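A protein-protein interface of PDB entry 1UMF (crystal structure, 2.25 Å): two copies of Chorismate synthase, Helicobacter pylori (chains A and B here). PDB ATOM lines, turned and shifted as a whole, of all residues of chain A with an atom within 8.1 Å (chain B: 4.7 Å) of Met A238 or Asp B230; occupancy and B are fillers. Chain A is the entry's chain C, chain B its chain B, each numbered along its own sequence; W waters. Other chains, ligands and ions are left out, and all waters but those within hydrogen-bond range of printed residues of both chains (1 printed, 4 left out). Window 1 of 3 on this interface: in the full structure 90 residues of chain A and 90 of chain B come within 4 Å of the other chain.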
ATOM      1  N   ARG A 132       1.007 -26.448 -27.527  1.00  0.00           N
ATOM      2  CA  ARG A 132       1.549 -25.095 -27.521  1.00  0.00           C
ATOM      3  C   ARG A 132       3.062 -25.049 -27.363  1.00  0.00           C
ATOM      4  O   ARG A 132       3.741 -24.306 -28.070  1.00  0.00           O
ATOM      5  CB  ARG A 132       0.903 -24.277 -26.406  1.00  0.00           C
ATOM      6  CG  ARG A 132      -0.504 -23.831 -26.707  1.00  0.00           C
ATOM      7  CD  ARG A 132      -1.227 -23.399 -25.438  1.00  0.00           C
ATOM      8  NE  ARG A 132      -2.578 -22.926 -25.726  1.00  0.00           N
ATOM      9  CZ  ARG A 132      -3.589 -22.953 -24.862  1.00  0.00           C
ATOM     10  NH1 ARG A 132      -4.779 -22.491 -25.226  1.00  0.00           N
ATOM     11  NH2 ARG A 132      -3.421 -23.457 -23.645  1.00  0.00           N
ATOM     12  N   ALA A 231      -1.940  -6.205 -27.984  1.00  0.00           N
ATOM     13  CA  ALA A 231      -3.296  -6.738 -28.083  1.00  0.00           C
ATOM     14  C   ALA A 231      -3.238  -8.245 -28.335  1.00  0.00           C
ATOM     15  O   ALA A 231      -3.987  -9.011 -27.729  1.00  0.00           O
ATOM     16  CB  ALA A 231      -4.058  -6.047 -29.214  1.00  0.00           C
ATOM     17  N   LYS A 232      -2.338  -8.664 -29.223  1.00  0.00           N
ATOM     18  CA  LYS A 232      -2.183 -10.080 -29.558  1.00  0.00           C
ATOM     19  C   LYS A 232      -1.501 -10.885 -28.457  1.00  0.00           C
ATOM     20  O   LYS A 232      -1.809 -12.063 -28.263  1.00  0.00           O
ATOM     21  CB  LYS A 232      -1.419 -10.230 -30.875  1.00  0.00           C
ATOM     22  CG  LYS A 232      -2.260  -9.883 -32.109  1.00  0.00           C
ATOM     23  CD  LYS A 232      -3.462 -10.827 -32.219  1.00  0.00           C
ATOM     24  CE  LYS A 232      -4.365 -10.501 -33.397  1.00  0.00           C
ATOM     25  NZ  LYS A 232      -5.488 -11.486 -33.485  1.00  0.00           N
ATOM     26  N   ILE A 233      -0.563 -10.265 -27.740  1.00  0.00           N
ATOM     27  CA  ILE A 233       0.087 -10.960 -26.629  1.00  0.00           C
ATOM     28  C   ILE A 233      -0.990 -11.158 -25.561  1.00  0.00           C
ATOM     29  O   ILE A 233      -1.104 -12.225 -24.962  1.00  0.00           O
ATOM     30  CB  ILE A 233       1.232 -10.128 -26.008  1.00  0.00           C
ATOM     31  CG1 ILE A 233       2.446 -10.143 -26.935  1.00  0.00           C
ATOM     32  CG2 ILE A 233       1.582 -10.672 -24.613  1.00  0.00           C
ATOM     33  CD1 ILE A 233       3.600  -9.281 -26.447  1.00  0.00           C
ATOM     34  N   ALA A 234      -1.787 -10.120 -25.341  1.00  0.00           N
ATOM     35  CA  ALA A 234      -2.855 -10.172 -24.348  1.00  0.00           C
ATOM     36  C   ALA A 234      -3.836 -11.299 -24.648  1.00  0.00           C
ATOM     37  O   ALA A 234      -4.291 -11.999 -23.743  1.00  0.00           O
ATOM     38  CB  ALA A 234      -3.595  -8.841 -24.310  1.00  0.00           C
ATOM     39  N   GLU A 235      -4.152 -11.461 -25.929  1.00  0.00           N
ATOM     40  CA  GLU A 235      -5.084 -12.482 -26.386  1.00  0.00           C
ATOM     41  C   GLU A 235      -4.586 -13.895 -26.101  1.00  0.00           C
ATOM     42  O   GLU A 235      -5.336 -14.749 -25.634  1.00  0.00           O
ATOM     43  CB  GLU A 235      -5.320 -12.321 -27.886  1.00  0.00           C
ATOM     44  CG  GLU A 235      -6.444 -13.171 -28.438  1.00  0.00           C
ATOM     45  CD  GLU A 235      -6.501 -13.120 -29.948  1.00  0.00           C
ATOM     46  OE1 GLU A 235      -5.606 -13.691 -30.604  1.00  0.00           O
ATOM     47  OE2 GLU A 235      -7.437 -12.497 -30.484  1.00  0.00           O
ATOM     48  N   ALA A 236      -3.319 -14.140 -26.392  1.00  0.00           N
ATOM     49  CA  ALA A 236      -2.745 -15.457 -26.169  1.00  0.00           C
ATOM     50  C   ALA A 236      -2.733 -15.803 -24.688  1.00  0.00           C
ATOM     51  O   ALA A 236      -3.246 -16.846 -24.282  1.00  0.00           O
ATOM     52  CB  ALA A 236      -1.324 -15.502 -26.726  1.00  0.00           C
ATOM     53  N   MET A 237      -2.153 -14.918 -23.880  1.00  0.00           N
ATOM     54  CA  MET A 237      -2.051 -15.152 -22.439  1.00  0.00           C
ATOM     55  C   MET A 237      -3.392 -15.333 -21.723  1.00  0.00           C
ATOM     56  O   MET A 237      -3.604 -16.338 -21.030  1.00  0.00           O
ATOM     57  CB  MET A 237      -1.282 -14.008 -21.767  1.00  0.00           C
ATOM     58  CG  MET A 237       0.048 -13.670 -22.426  1.00  0.00           C
ATOM     59  SD  MET A 237       1.191 -15.063 -22.481  1.00  0.00           S
ATOM     60  CE  MET A 237       2.556 -14.343 -23.372  1.00  0.00           C
ATOM     61  N   MET A 238      -4.290 -14.364 -21.883  1.00  0.00           N
ATOM     62  CA  MET A 238      -5.590 -14.423 -21.213  1.00  0.00           C
ATOM     63  C   MET A 238      -6.354 -15.684 -21.601  1.00  0.00           C
ATOM     64  O   MET A 238      -7.220 -16.145 -20.857  1.00  0.00           O
ATOM     65  CB  MET A 238      -6.424 -13.181 -21.544  1.00  0.00           C
ATOM     66  CG  MET A 238      -7.682 -13.013 -20.690  1.00  0.00           C
ATOM     67  SD  MET A 238      -7.368 -12.515 -18.976  1.00  0.00           S
ATOM     68  CE  MET A 238      -7.105 -10.759 -19.160  1.00  0.00           C
ATOM     69  N   GLY A 239      -6.026 -16.237 -22.762  1.00  0.00           N
ATOM     70  CA  GLY A 239      -6.688 -17.442 -23.215  1.00  0.00           C
ATOM     71  C   GLY A 239      -6.202 -18.695 -22.501  1.00  0.00           C
ATOM     72  O   GLY A 239      -6.765 -19.777 -22.678  1.00  0.00           O
ATOM     73  N   LEU A 240      -5.144 -18.574 -21.708  1.00  0.00           N
ATOM     74  CA  LEU A 240      -4.650 -19.731 -20.976  1.00  0.00           C
ATOM     75  C   LEU A 240      -5.583 -19.861 -19.768  1.00  0.00           C
ATOM     76  O   LEU A 240      -5.880 -18.870 -19.099  1.00  0.00           O
ATOM     77  CB  LEU A 240      -3.203 -19.498 -20.537  1.00  0.00           C
ATOM     78  CG  LEU A 240      -2.362 -20.687 -20.065  1.00  0.00           C
ATOM     79  CD1 LEU A 240      -0.951 -20.210 -19.745  1.00  0.00           C
ATOM     80  CD2 LEU A 240      -2.982 -21.318 -18.834  1.00  0.00           C
ATOM     81  N   ASN A 241      -6.063 -21.067 -19.495  1.00  0.00           N
ATOM     82  CA  ASN A 241      -6.978 -21.259 -18.376  1.00  0.00           C
ATOM     83  C   ASN A 241      -6.340 -20.903 -17.027  1.00  0.00           C
ATOM     84  O   ASN A 241      -5.220 -21.313 -16.731  1.00  0.00           O
ATOM     85  CB  ASN A 241      -7.487 -22.701 -18.347  1.00  0.00           C
ATOM     86  CG  ASN A 241      -8.624 -22.894 -17.360  1.00  0.00           C
ATOM     87  OD1 ASN A 241      -8.525 -23.697 -16.426  1.00  0.00           O
ATOM     88  ND2 ASN A 241      -9.716 -22.154 -17.559  1.00  0.00           N
ATOM     89  N   GLY A 242      -7.068 -20.141 -16.216  1.00  0.00           N
ATOM     90  CA  GLY A 242      -6.559 -19.731 -14.922  1.00  0.00           C
ATOM     91  C   GLY A 242      -6.059 -18.293 -14.926  1.00  0.00           C
ATOM     92  O   GLY A 242      -5.979 -17.650 -13.881  1.00  0.00           O
ATOM     93  N   VAL A 243      -5.711 -17.783 -16.103  1.00  0.00           N
ATOM     94  CA  VAL A 243      -5.218 -16.416 -16.224  1.00  0.00           C
ATOM     95  C   VAL A 243      -6.382 -15.440 -16.080  1.00  0.00           C
ATOM     96  O   VAL A 243      -7.396 -15.584 -16.757  1.00  0.00           O
ATOM     97  CB  VAL A 243      -4.516 -16.219 -17.579  1.00  0.00           C
ATOM     98  CG1 VAL A 243      -4.144 -14.749 -17.782  1.00  0.00           C
ATOM     99  CG2 VAL A 243      -3.272 -17.104 -17.634  1.00  0.00           C
ATOM    100  N   LYS A 244      -6.239 -14.461 -15.187  1.00  0.00           N
ATOM    101  CA  LYS A 244      -7.295 -13.478 -14.944  1.00  0.00           C
ATOM    102  C   LYS A 244      -6.873 -12.035 -15.236  1.00  0.00           C
ATOM    103  O   LYS A 244      -7.700 -11.120 -15.193  1.00  0.00           O
ATOM    104  CB  LYS A 244      -7.786 -13.576 -13.493  1.00  0.00           C
ATOM    105  CG  LYS A 244      -8.257 -14.972 -13.071  1.00  0.00           C
ATOM    106  CD  LYS A 244      -9.386 -15.495 -13.966  1.00  0.00           C
ATOM    107  CE  LYS A 244     -10.615 -14.593 -13.936  1.00  0.00           C
ATOM    108  NZ  LYS A 244     -11.680 -15.130 -14.848  1.00  0.00           N
ATOM    109  N   ALA A 245      -5.592 -11.835 -15.523  1.00  0.00           N
ATOM    110  CA  ALA A 245      -5.080 -10.505 -15.834  1.00  0.00           C
ATOM    111  C   ALA A 245      -3.752 -10.604 -16.576  1.00  0.00           C
ATOM    112  O   ALA A 245      -2.984 -11.546 -16.370  1.00  0.00           O
ATOM    113  CB  ALA A 245      -4.907  -9.688 -14.557  1.00  0.00           C
ATOM    114  N   VAL A 246      -3.498  -9.635 -17.451  1.00  0.00           N
ATOM    115  CA  VAL A 246      -2.261  -9.585 -18.226  1.00  0.00           C
ATOM    116  C   VAL A 246      -1.721  -8.163 -18.163  1.00  0.00           C
ATOM    117  O   VAL A 246      -2.468  -7.200 -18.311  1.00  0.00           O
ATOM    118  CB  VAL A 246      -2.502  -9.963 -19.712  1.00  0.00           C
ATOM    119  CG1 VAL A 246      -1.199  -9.909 -20.481  1.00  0.00           C
ATOM    120  CG2 VAL A 246      -3.120 -11.341 -19.803  1.00  0.00           C
ATOM    121  N   GLU A 247      -0.418  -8.039 -17.946  1.00  0.00           N
ATOM    122  CA  GLU A 247       0.224  -6.734 -17.843  1.00  0.00           C
ATOM    123  C   GLU A 247       1.352  -6.545 -18.844  1.00  0.00           C
ATOM    124  O   GLU A 247       2.139  -7.459 -19.084  1.00  0.00           O
ATOM    125  CB  GLU A 247       0.803  -6.543 -16.439  1.00  0.00           C
ATOM    126  CG  GLU A 247      -0.213  -6.339 -15.326  1.00  0.00           C
ATOM    127  CD  GLU A 247       0.469  -6.053 -14.006  1.00  0.00           C
ATOM    128  OE1 GLU A 247       0.724  -7.005 -13.237  1.00  0.00           O
ATOM    129  OE2 GLU A 247       0.776  -4.873 -13.747  1.00  0.00           O
ATOM    130  N   VAL A 291       6.038  -8.846 -20.014  1.00  0.00           N
ATOM    131  CA  VAL A 291       4.658  -9.280 -19.814  1.00  0.00           C
ATOM    132  C   VAL A 291       4.477 -10.002 -18.480  1.00  0.00           C
ATOM    133  O   VAL A 291       5.266 -10.884 -18.130  1.00  0.00           O
ATOM    134  CB  VAL A 291       4.203 -10.248 -20.946  1.00  0.00           C
ATOM    135  CG1 VAL A 291       2.708 -10.521 -20.834  1.00  0.00           C
ATOM    136  CG2 VAL A 291       4.535  -9.663 -22.308  1.00  0.00           C
ATOM    137  N   VAL A 293       1.706 -12.201 -16.212  1.00  0.00           N
ATOM    138  CA  VAL A 293       0.471 -12.977 -16.299  1.00  0.00           C
ATOM    139  C   VAL A 293       0.026 -13.460 -14.917  1.00  0.00           C
ATOM    140  O   VAL A 293       0.783 -14.123 -14.203  1.00  0.00           O
ATOM    141  CB  VAL A 293       0.669 -14.196 -17.241  1.00  0.00           C
ATOM    142  CG1 VAL A 293      -0.650 -14.900 -17.483  1.00  0.00           C
ATOM    143  CG2 VAL A 293       1.275 -13.736 -18.560  1.00  0.00           C
ATOM    144  N   HIS A 294      -1.204 -13.115 -14.552  1.00  0.00           N
ATOM    145  CA  HIS A 294      -1.772 -13.482 -13.258  1.00  0.00           C
ATOM    146  C   HIS A 294      -2.637 -14.738 -13.301  1.00  0.00           C
ATOM    147  O   HIS A 294      -3.597 -14.808 -14.061  1.00  0.00           O
ATOM    148  CB  HIS A 294      -2.617 -12.324 -12.704  1.00  0.00           C
ATOM    149  CG  HIS A 294      -1.811 -11.142 -12.271  1.00  0.00           C
ATOM    150  ND1 HIS A 294      -1.181 -10.301 -13.164  1.00  0.00           N
ATOM    151  CD2 HIS A 294      -1.490 -10.690 -11.035  1.00  0.00           C
ATOM    152  CE1 HIS A 294      -0.505  -9.384 -12.497  1.00  0.00           C
ATOM    153  NE2 HIS A 294      -0.676  -9.597 -11.204  1.00  0.00           N
ATOM    154  N   CYS A 335       3.243 -19.690 -21.398  1.00  0.00           N
ATOM    155  CA  CYS A 335       3.167 -18.285 -21.797  1.00  0.00           C
ATOM    156  C   CYS A 335       4.375 -17.920 -22.643  1.00  0.00           C
ATOM    157  O   CYS A 335       4.267 -17.164 -23.608  1.00  0.00           O
ATOM    158  CB  CYS A 335       3.107 -17.372 -20.568  1.00  0.00           C
ATOM    159  SG  CYS A 335       1.551 -17.474 -19.653  1.00  0.00           S
ATOM    160  N   LEU A 338       3.815 -19.181 -26.041  1.00  0.00           N
ATOM    161  CA  LEU A 338       2.807 -18.360 -26.693  1.00  0.00           C
ATOM    162  C   LEU A 338       3.405 -17.041 -27.145  1.00  0.00           C
ATOM    163  O   LEU A 338       3.061 -16.537 -28.214  1.00  0.00           O
ATOM    164  CB  LEU A 338       1.625 -18.116 -25.752  1.00  0.00           C
ATOM    165  CG  LEU A 338       0.784 -19.364 -25.479  1.00  0.00           C
ATOM    166  CD1 LEU A 338      -0.246 -19.090 -24.397  1.00  0.00           C
ATOM    167  CD2 LEU A 338       0.101 -19.783 -26.770  1.00  0.00           C
ATOM    168  N   LYS B 228     -11.589 -17.582 -27.075  1.00  0.00           N
ATOM    169  CA  LYS B 228     -12.313 -17.576 -25.801  1.00  0.00           C
ATOM    170  C   LYS B 228     -12.803 -16.158 -25.536  1.00  0.00           C
ATOM    171  O   LYS B 228     -12.176 -15.186 -25.971  1.00  0.00           O
ATOM    172  CB  LYS B 228     -11.402 -18.022 -24.652  1.00  0.00           C
ATOM    173  CG  LYS B 228     -11.050 -19.505 -24.663  1.00  0.00           C
ATOM    174  CD  LYS B 228     -10.094 -19.868 -23.529  1.00  0.00           C
ATOM    175  CE  LYS B 228      -9.867 -21.380 -23.463  1.00  0.00           C
ATOM    176  NZ  LYS B 228      -8.785 -21.749 -22.497  1.00  0.00           N
ATOM    177  N   LEU B 229     -13.910 -16.045 -24.811  1.00  0.00           N
ATOM    178  CA  LEU B 229     -14.498 -14.746 -24.503  1.00  0.00           C
ATOM    179  C   LEU B 229     -13.539 -13.787 -23.809  1.00  0.00           C
ATOM    180  O   LEU B 229     -13.386 -12.643 -24.240  1.00  0.00           O
ATOM    181  CB  LEU B 229     -15.751 -14.932 -23.646  1.00  0.00           C
ATOM    182  CG  LEU B 229     -16.489 -13.673 -23.178  1.00  0.00           C
ATOM    183  CD1 LEU B 229     -16.806 -12.765 -24.359  1.00  0.00           C
ATOM    184  CD2 LEU B 229     -17.765 -14.091 -22.460  1.00  0.00           C
ATOM    185  N   ASP B 230     -12.889 -14.241 -22.743  1.00  0.00           N
ATOM    186  CA  ASP B 230     -11.966 -13.369 -22.030  1.00  0.00           C
ATOM    187  C   ASP B 230     -10.750 -13.008 -22.878  1.00  0.00           C
ATOM    188  O   ASP B 230     -10.223 -11.901 -22.784  1.00  0.00           O
ATOM    189  CB  ASP B 230     -11.547 -13.992 -20.685  1.00  0.00           C
ATOM    190  CG  ASP B 230     -11.094 -15.440 -20.804  1.00  0.00           C
ATOM    191  OD1 ASP B 230     -11.228 -16.044 -21.891  1.00  0.00           O
ATOM    192  OD2 ASP B 230     -10.610 -15.983 -19.785  1.00  0.00           O
ATOM    193  N   ALA B 231     -10.318 -13.938 -23.719  1.00  0.00           N
ATOM    194  CA  ALA B 231      -9.176 -13.694 -24.593  1.00  0.00           C
ATOM    195  C   ALA B 231      -9.487 -12.552 -25.567  1.00  0.00           C
ATOM    196  O   ALA B 231      -8.648 -11.683 -25.802  1.00  0.00           O
ATOM    197  CB  ALA B 231      -8.831 -14.964 -25.375  1.00  0.00           C
ATOM    198  N   LYS B 232     -10.692 -12.565 -26.135  1.00  0.00           N
ATOM    199  CA  LYS B 232     -11.108 -11.535 -27.086  1.00  0.00           C
ATOM    200  C   LYS B 232     -11.405 -10.195 -26.411  1.00  0.00           C
ATOM    201  O   LYS B 232     -11.248  -9.130 -27.015  1.00  0.00           O
ATOM    202  CB  LYS B 232     -12.330 -12.015 -27.881  1.00  0.00           C
ATOM    203  CG  LYS B 232     -12.005 -13.084 -28.930  1.00  0.00           C
ATOM    204  CD  LYS B 232     -11.043 -12.538 -29.990  1.00  0.00           C
ATOM    205  CE  LYS B 232     -10.570 -13.622 -30.948  1.00  0.00           C
ATOM    206  NZ  LYS B 232      -9.587 -13.099 -31.943  1.00  0.00           N
ATOM    207  N   ILE B 233     -11.857 -10.238 -25.165  1.00  0.00           N
ATOM    208  CA  ILE B 233     -12.112  -8.999 -24.456  1.00  0.00           C
ATOM    209  C   ILE B 233     -10.738  -8.374 -24.246  1.00  0.00           C
ATOM    210  O   ILE B 233     -10.512  -7.211 -24.592  1.00  0.00           O
ATOM    211  CB  ILE B 233     -12.803  -9.254 -23.089  1.00  0.00           C
ATOM    212  CG1 ILE B 233     -14.283  -9.586 -23.319  1.00  0.00           C
ATOM    213  CG2 ILE B 233     -12.649  -8.024 -22.183  1.00  0.00           C
ATOM    214  CD1 ILE B 233     -15.056  -9.961 -22.063  1.00  0.00           C
ATOM    215  N   ALA B 234      -9.814  -9.166 -23.708  1.00  0.00           N
ATOM    216  CA  ALA B 234      -8.463  -8.688 -23.453  1.00  0.00           C
ATOM    217  C   ALA B 234      -7.821  -8.103 -24.709  1.00  0.00           C
ATOM    218  O   ALA B 234      -7.213  -7.028 -24.661  1.00  0.00           O
ATOM    219  CB  ALA B 234      -7.602  -9.822 -22.904  1.00  0.00           C
ATOM    220  N   VAL B 246      -5.155  -5.492 -18.442  1.00  0.00           N
ATOM    221  CA  VAL B 246      -6.566  -5.800 -18.497  1.00  0.00           C
ATOM    222  C   VAL B 246      -6.816  -6.864 -17.449  1.00  0.00           C
ATOM    223  O   VAL B 246      -6.037  -7.809 -17.323  1.00  0.00           O
ATOM    224  CB  VAL B 246      -6.961  -6.357 -19.881  1.00  0.00           C
ATOM    225  CG1 VAL B 246      -8.465  -6.563 -19.950  1.00  0.00           C
ATOM    226  CG2 VAL B 246      -6.495  -5.416 -20.970  1.00  0.00           C
ATOM    227  N   ILE B 248      -9.955  -9.386 -15.528  1.00  0.00           N
ATOM    228  CA  ILE B 248     -11.293  -9.955 -15.648  1.00  0.00           C
ATOM    229  C   ILE B 248     -11.706 -10.377 -14.233  1.00  0.00           C
ATOM    230  O   ILE B 248     -10.996 -11.134 -13.578  1.00  0.00           O
ATOM    231  CB  ILE B 248     -11.326 -11.206 -16.571  1.00  0.00           C
ATOM    232  CG1 ILE B 248     -10.831 -10.854 -17.985  1.00  0.00           C
ATOM    233  CG2 ILE B 248     -12.753 -11.759 -16.637  1.00  0.00           C
ATOM    234  CD1 ILE B 248     -11.713  -9.874 -18.727  1.00  0.00           C
ATOM    235  N   VAL B 279     -16.739 -15.011 -16.681  1.00  0.00           N
ATOM    236  CA  VAL B 279     -16.098 -15.874 -17.667  1.00  0.00           C
ATOM    237  C   VAL B 279     -15.355 -17.037 -17.013  1.00  0.00           C
ATOM    238  O   VAL B 279     -14.421 -16.828 -16.243  1.00  0.00           O
ATOM    239  CB  VAL B 279     -15.085 -15.075 -18.526  1.00  0.00           C
ATOM    240  CG1 VAL B 279     -14.536 -15.961 -19.643  1.00  0.00           C
ATOM    241  CG2 VAL B 279     -15.749 -13.821 -19.098  1.00  0.00           C
ATOM    242  N   GLY B 282     -12.893 -19.857 -20.294  1.00  0.00           N
ATOM    243  CA  GLY B 282     -12.906 -19.155 -21.563  1.00  0.00           C
ATOM    244  C   GLY B 282     -14.307 -18.845 -22.060  1.00  0.00           C
ATOM    245  O   GLY B 282     -14.457 -18.226 -23.105  1.00  0.00           O
HETATM  246  O   HOH W   1     -10.305 -14.674 -17.159  1.00  0.00           O
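The side-chain amino group (NZ) of Lys B228 is in hydrogen-bond range of the backbone carbonyl oxygen (O) of Gly A239 (2.8 Å). OE2 of Glu A235 lies within salt-bridge range of NZ of Lys B232 (2.7 Å). O of Val B246 is in hydrogen-bond range of N of Val A246, at 3.1 Å. O of Lys A244 lies within hydrogen-bond range of N of Ile B248 (2.9 Å).
NZ of Lys A232 lies within salt-bridge range of OE1 of Glu A235, at 3.6 Å. The backbone NH (N) of Lys A244 is in hydrogen-bond range of the backbone carbonyl oxygen (O) of His A294 (2.9 Å). O of Ala A245 is in hydrogen-bond range of N of His A294 (3.0 Å).
Glu A235 touches Ala B231. Asp B230 touches Met A238. Met A238 touches Ala B234 (CB to CB, 3.8 Å). O of Val B246 touches CE of Met A238 (3.6 Å). Met A238 touches Ile B248. CB of Ala B231 touches CA of Gly A239 (3.9 Å). O of Val B279 touches NZ of Lys A244 (3.5 Å). Val B246 touches Ala A245 (O to CA, 3.2 Å).
Lys A232 touches none of the printed residues of chain B. Printed residues of chain B within 4 Å of Glu A235: Ala B231 (3.5 Å) and Lys B232 (2.7 Å). Of the printed residues of chain B, Met A238 touches Asp B230, Ala B234, Val B246 and Ile B248. Printed residues of chain B within 4 Å of Gly A239: Lys B228 and Ala B231. Gly A242 touches none of the printed residues of chain B. Of the printed residues of chain B, Ala A245 touches Val B246 (3.2 Å). Printed residues of chain B within 4 Å of Val A246: Val B246. Of the printed residues of chain A, Asp B230 touches Met A238. Ala B231 touches just these residues of chain A: Glu A235 and Gly A239. Of the printed residues of chain A, Ile B248 touches Met A238 (3.9 Å) and Lys A244 (2.9 Å). The nearest printed residue of chain B that does not touch Lys A244 is Val B246 (4.3 Å).
Hydrophobic or aromatic side chains of chain A within 4 Å of the printed part of chain B: Met A238 and Ala A245. Along chain B the printed residues that touch a printed residue of chain A span positions 228 to 279. Among the printed residues, Asp or Glu carboxylates within 4 Å of a Lys or Arg side-chain nitrogen of the other chain: Glu A235 with Lys B232.
Val A246 touches its own counterpart, Val B246.
Water W1 lies within hydrogen-bond range of NZ of Lys A244 (2.7 Å), OD2 of Asp B230 (2.9 Å) and O of Val A243 (3.1 Å).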
